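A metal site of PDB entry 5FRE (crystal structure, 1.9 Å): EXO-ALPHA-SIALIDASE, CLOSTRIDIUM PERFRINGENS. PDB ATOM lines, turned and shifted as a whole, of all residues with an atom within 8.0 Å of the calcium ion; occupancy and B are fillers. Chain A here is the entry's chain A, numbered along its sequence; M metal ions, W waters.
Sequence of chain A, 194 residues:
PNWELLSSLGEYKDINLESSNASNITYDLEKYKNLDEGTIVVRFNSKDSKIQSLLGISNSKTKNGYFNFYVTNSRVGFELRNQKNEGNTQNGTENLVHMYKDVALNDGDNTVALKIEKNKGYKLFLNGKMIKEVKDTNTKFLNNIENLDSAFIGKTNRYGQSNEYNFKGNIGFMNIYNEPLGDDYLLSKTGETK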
ATOM      1  N   PHE A  44     -22.058  18.878 -20.357  1.00  0.00           N
ATOM      2  CA  PHE A  44     -22.752  19.916 -19.604  1.00  0.00           C
ATOM      3  C   PHE A  44     -21.782  20.622 -18.642  1.00  0.00           C
ATOM      4  O   PHE A  44     -20.752  20.073 -18.254  1.00  0.00           O
ATOM      5  CB  PHE A  44     -23.936  19.320 -18.850  1.00  0.00           C
ATOM      6  CG  PHE A  44     -23.552  18.420 -17.687  1.00  0.00           C
ATOM      7  CD1 PHE A  44     -23.349  17.073 -17.884  1.00  0.00           C
ATOM      8  CD2 PHE A  44     -23.397  18.941 -16.395  1.00  0.00           C
ATOM      9  CE1 PHE A  44     -22.947  16.230 -16.836  1.00  0.00           C
ATOM     10  CE2 PHE A  44     -23.015  18.117 -15.325  1.00  0.00           C
ATOM     11  CZ  PHE A  44     -22.814  16.742 -15.551  1.00  0.00           C
ATOM     12  N   ASN A  45     -22.153  21.827 -18.260  1.00  0.00           N
ATOM     13  CA  ASN A  45     -21.411  22.644 -17.280  1.00  0.00           C
ATOM     14  C   ASN A  45     -22.393  23.520 -16.532  1.00  0.00           C
ATOM     15  O   ASN A  45     -22.823  24.544 -17.025  1.00  0.00           O
ATOM     16  CB  ASN A  45     -20.305  23.505 -17.927  1.00  0.00           C
ATOM     17  CG  ASN A  45     -19.445  24.218 -16.904  1.00  0.00           C
ATOM     18  OD1 ASN A  45     -19.605  24.072 -15.676  1.00  0.00           O
ATOM     19  ND2 ASN A  45     -18.471  24.941 -17.402  1.00  0.00           N
ATOM     20  N   SER A  46     -22.740  23.071 -15.338  1.00  0.00           N
ATOM     21  CA  SER A  46     -23.653  23.757 -14.473  1.00  0.00           C
ATOM     22  C   SER A  46     -22.886  24.737 -13.591  1.00  0.00           C
ATOM     23  O   SER A  46     -21.757  24.473 -13.219  1.00  0.00           O
ATOM     24  CB  SER A  46     -24.378  22.787 -13.549  1.00  0.00           C
ATOM     25  OG  SER A  46     -25.357  23.511 -12.815  1.00  0.00           O
ATOM     26  N   LYS A  47     -23.588  25.786 -13.184  1.00  0.00           N
ATOM     27  CA  LYS A  47     -23.121  26.798 -12.248  1.00  0.00           C
ATOM     28  C   LYS A  47     -23.909  26.780 -10.920  1.00  0.00           C
ATOM     29  O   LYS A  47     -23.699  27.648 -10.105  1.00  0.00           O
ATOM     30  CB  LYS A  47     -23.304  28.193 -12.886  1.00  0.00           C
ATOM     31  N   ASP A  48     -24.808  25.819 -10.685  1.00  0.00           N
ATOM     32  CA  ASP A  48     -25.574  25.751  -9.430  1.00  0.00           C
ATOM     33  C   ASP A  48     -25.460  24.359  -8.819  1.00  0.00           C
ATOM     34  O   ASP A  48     -25.038  23.413  -9.485  1.00  0.00           O
ATOM     35  CB  ASP A  48     -27.054  26.142  -9.633  1.00  0.00           C
ATOM     36  CG  ASP A  48     -27.699  26.763  -8.370  1.00  0.00           C
ATOM     37  OD1 ASP A  48     -27.557  26.234  -7.239  1.00  0.00           O
ATOM     38  OD2 ASP A  48     -28.348  27.806  -8.471  1.00  0.00           O
ATOM     39  N   ASN A  73     -24.393  19.570  -8.137  1.00  0.00           N
ATOM     40  CA  ASN A  73     -22.903  19.667  -8.135  1.00  0.00           C
ATOM     41  C   ASN A  73     -22.144  18.440  -7.627  1.00  0.00           C
ATOM     42  O   ASN A  73     -20.924  18.413  -7.699  1.00  0.00           O
ATOM     43  CB  ASN A  73     -22.435  20.888  -7.350  1.00  0.00           C
ATOM     44  CG  ASN A  73     -22.836  20.832  -5.903  1.00  0.00           C
ATOM     45  OD1 ASN A  73     -23.791  20.145  -5.496  1.00  0.00           O
ATOM     46  ND2 ASN A  73     -22.121  21.588  -5.098  1.00  0.00           N
ATOM     47  N   LEU A 105     -17.757  16.028  -9.450  1.00  0.00           N
ATOM     48  CA  LEU A 105     -17.889  16.621 -10.770  1.00  0.00           C
ATOM     49  C   LEU A 105     -16.747  17.614 -11.076  1.00  0.00           C
ATOM     50  O   LEU A 105     -16.192  18.189 -10.189  1.00  0.00           O
ATOM     51  CB  LEU A 105     -19.268  17.255 -10.918  1.00  0.00           C
ATOM     52  CG  LEU A 105     -20.355  16.184 -11.079  1.00  0.00           C
ATOM     53  CD1 LEU A 105     -21.714  16.757 -10.757  1.00  0.00           C
ATOM     54  CD2 LEU A 105     -20.383  15.599 -12.479  1.00  0.00           C
ATOM     55  N   ASN A 106     -16.402  17.775 -12.353  1.00  0.00           N
ATOM     56  CA  ASN A 106     -15.446  18.841 -12.767  1.00  0.00           C
ATOM     57  C   ASN A 106     -16.046  20.199 -12.578  1.00  0.00           C
ATOM     58  O   ASN A 106     -17.235  20.349 -12.766  1.00  0.00           O
ATOM     59  CB  ASN A 106     -15.098  18.741 -14.261  1.00  0.00           C
ATOM     60  CG  ASN A 106     -14.451  17.425 -14.637  1.00  0.00           C
ATOM     61  OD1 ASN A 106     -14.665  16.896 -15.750  1.00  0.00           O
ATOM     62  ND2 ASN A 106     -13.667  16.903 -13.736  1.00  0.00           N
ATOM     63  N   ASP A 107     -15.223  21.210 -12.238  1.00  0.00           N
ATOM     64  CA  ASP A 107     -15.704  22.605 -12.254  1.00  0.00           C
ATOM     65  C   ASP A 107     -16.230  23.076 -13.643  1.00  0.00           C
ATOM     66  O   ASP A 107     -17.175  23.894 -13.700  1.00  0.00           O
ATOM     67  CB  ASP A 107     -14.591  23.596 -11.812  1.00  0.00           C
ATOM     68  CG  ASP A 107     -14.122  23.350 -10.374  1.00  0.00           C
ATOM     69  OD1 ASP A 107     -14.909  22.838  -9.553  1.00  0.00           O
ATOM     70  OD2 ASP A 107     -12.951  23.682 -10.068  1.00  0.00           O
ATOM     71  N   GLY A 108     -15.578  22.639 -14.714  1.00  0.00           N
ATOM     72  CA  GLY A 108     -15.954  22.994 -16.085  1.00  0.00           C
ATOM     73  C   GLY A 108     -16.808  21.881 -16.692  1.00  0.00           C
ATOM     74  O   GLY A 108     -17.696  21.366 -16.024  1.00  0.00           O
ATOM     75  N   ASP A 109     -16.513  21.497 -17.923  1.00  0.00           N
ATOM     76  CA  ASP A 109     -17.319  20.484 -18.658  1.00  0.00           C
ATOM     77  C   ASP A 109     -17.290  19.097 -18.018  1.00  0.00           C
ATOM     78  O   ASP A 109     -16.266  18.637 -17.543  1.00  0.00           O
ATOM     79  CB  ASP A 109     -16.905  20.427 -20.129  1.00  0.00           C
ATOM     80  CG  ASP A 109     -17.484  21.598 -20.949  1.00  0.00           C
ATOM     81  OD1 ASP A 109     -18.468  22.241 -20.493  1.00  0.00           O
ATOM     82  OD2 ASP A 109     -16.975  21.883 -22.062  1.00  0.00           O
ATOM     83  N   ASN A 110     -18.459  18.463 -17.966  1.00  0.00           N
ATOM     84  CA  ASN A 110     -18.579  17.052 -17.598  1.00  0.00           C
ATOM     85  C   ASN A 110     -19.387  16.342 -18.691  1.00  0.00           C
ATOM     86  O   ASN A 110     -20.190  16.976 -19.392  1.00  0.00           O
ATOM     87  CB  ASN A 110     -19.311  16.900 -16.268  1.00  0.00           C
ATOM     88  CG  ASN A 110     -18.526  17.446 -15.099  1.00  0.00           C
ATOM     89  OD1 ASN A 110     -17.586  16.795 -14.582  1.00  0.00           O
ATOM     90  ND2 ASN A 110     -18.906  18.657 -14.650  1.00  0.00           N
ATOM     91  N   PHE A 167     -32.024  24.129 -15.207  1.00  0.00           N
ATOM     92  CA  PHE A 167     -30.606  24.077 -15.328  1.00  0.00           C
ATOM     93  C   PHE A 167     -30.089  25.497 -15.513  1.00  0.00           C
ATOM     94  O   PHE A 167     -30.701  26.296 -16.250  1.00  0.00           O
ATOM     95  CB  PHE A 167     -30.232  23.252 -16.558  1.00  0.00           C
ATOM     96  CG  PHE A 167     -28.774  22.928 -16.677  1.00  0.00           C
ATOM     97  CD1 PHE A 167     -27.887  23.798 -17.290  1.00  0.00           C
ATOM     98  CD2 PHE A 167     -28.284  21.711 -16.218  1.00  0.00           C
ATOM     99  CE1 PHE A 167     -26.551  23.485 -17.408  1.00  0.00           C
ATOM    100  CE2 PHE A 167     -26.921  21.389 -16.318  1.00  0.00           C
ATOM    101  CZ  PHE A 167     -26.061  22.268 -16.949  1.00  0.00           C
ATOM    102  N   LYS A 168     -28.970  25.764 -14.878  1.00  0.00           N
ATOM    103  CA  LYS A 168     -28.228  27.010 -15.069  1.00  0.00           C
ATOM    104  C   LYS A 168     -26.799  26.697 -15.464  1.00  0.00           C
ATOM    105  O   LYS A 168     -26.034  26.074 -14.700  1.00  0.00           O
ATOM    106  CB  LYS A 168     -28.241  27.879 -13.794  1.00  0.00           C
ATOM    107  CG  LYS A 168     -27.583  29.245 -14.024  1.00  0.00           C
ATOM    108  CD  LYS A 168     -28.232  30.375 -13.255  1.00  0.00           C
ATOM    109  CE  LYS A 168     -27.689  31.733 -13.695  1.00  0.00           C
ATOM    110  NZ  LYS A 168     -28.840  32.547 -14.178  1.00  0.00           N
ATOM    111  N   GLY A 169     -26.449  27.104 -16.668  1.00  0.00           N
ATOM    112  CA  GLY A 169     -25.117  26.930 -17.197  1.00  0.00           C
ATOM    113  C   GLY A 169     -25.217  26.751 -18.693  1.00  0.00           C
ATOM    114  O   GLY A 169     -26.002  27.447 -19.361  1.00  0.00           O
ATOM    115  N   ASN A 170     -24.405  25.834 -19.246  1.00  0.00           N
ATOM    116  CA  ASN A 170     -24.544  25.478 -20.637  1.00  0.00           C
ATOM    117  C   ASN A 170     -24.470  23.952 -20.893  1.00  0.00           C
ATOM    118  O   ASN A 170     -23.826  23.220 -20.150  1.00  0.00           O
ATOM    119  CB  ASN A 170     -23.556  26.247 -21.513  1.00  0.00           C
ATOM    120  CG  ASN A 170     -22.191  25.628 -21.526  1.00  0.00           C
ATOM    121  OD1 ASN A 170     -21.872  24.832 -22.414  1.00  0.00           O
ATOM    122  ND2 ASN A 170     -21.361  25.984 -20.557  1.00  0.00           N
HETATM  123 CA    CA M   1     -19.475  24.347 -13.360  1.00  0.00          CA
HETATM  124  O   HOH W   1     -19.404  23.354 -11.111  1.00  0.00           O
HETATM  125  O   HOH W   2     -19.351  26.343 -11.897  1.00  0.00           O
HETATM  126  O   HOH W   3     -19.205  21.974 -13.882  1.00  0.00           O
HETATM  127  O   HOH W   4     -19.371  26.595 -14.200  1.00  0.00           O
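Water W3 lies within hydrogen-bond range of the backbone carbonyl oxygen of Gly 108 (2.7 Å), the backbone carbonyl oxygen of Asn 106 (2.8 Å) and the side-chain amide nitrogen of Asn 110 (3.4 Å).
Within 4 Å of the calcium ion: Asn 45, Ser 46 and Asp 107. Along chain A the residues within 4 Å of the calcium ion span positions 45 to 107. The nearest printed residue that does not touch the calcium ion is Lys 47 (4.4 Å).
The calcium ion is bound by the backbone carbonyl oxygen (O) of Ser 46 (2.3 Å), the side-chain amide oxygen (OD1) of Asn 45 (2.3 Å), the backbone carbonyl oxygen (O) of Asp 107 (2.4 Å), water W4 (2.4 Å), water W3 (2.4 Å), water W1 (2.5 Å) and water W2 (2.5 Å). The calcium ion has seven donor atoms within binding distance.
The side-chain hydroxyl (OG) of Ser 46 sits at hydrogen-bond distance from the backbone carbonyl oxygen (O) of Lys 168 (3.3 Å). The backbone carbonyl oxygen of Asn 170 sits at hydrogen-bond distance from the backbone NH of Asn 45 (2.9 Å). The side-chain hydroxyl (OG) of Ser 46 sits at hydrogen-bond distance from the backbone NH (N) of Asp 48, at 3.2 Å. The side-chain amide oxygen (OD1) of Asn 45 lies close to the backbone carbonyl oxygen (O) of Gly 108 (3.3 Å).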
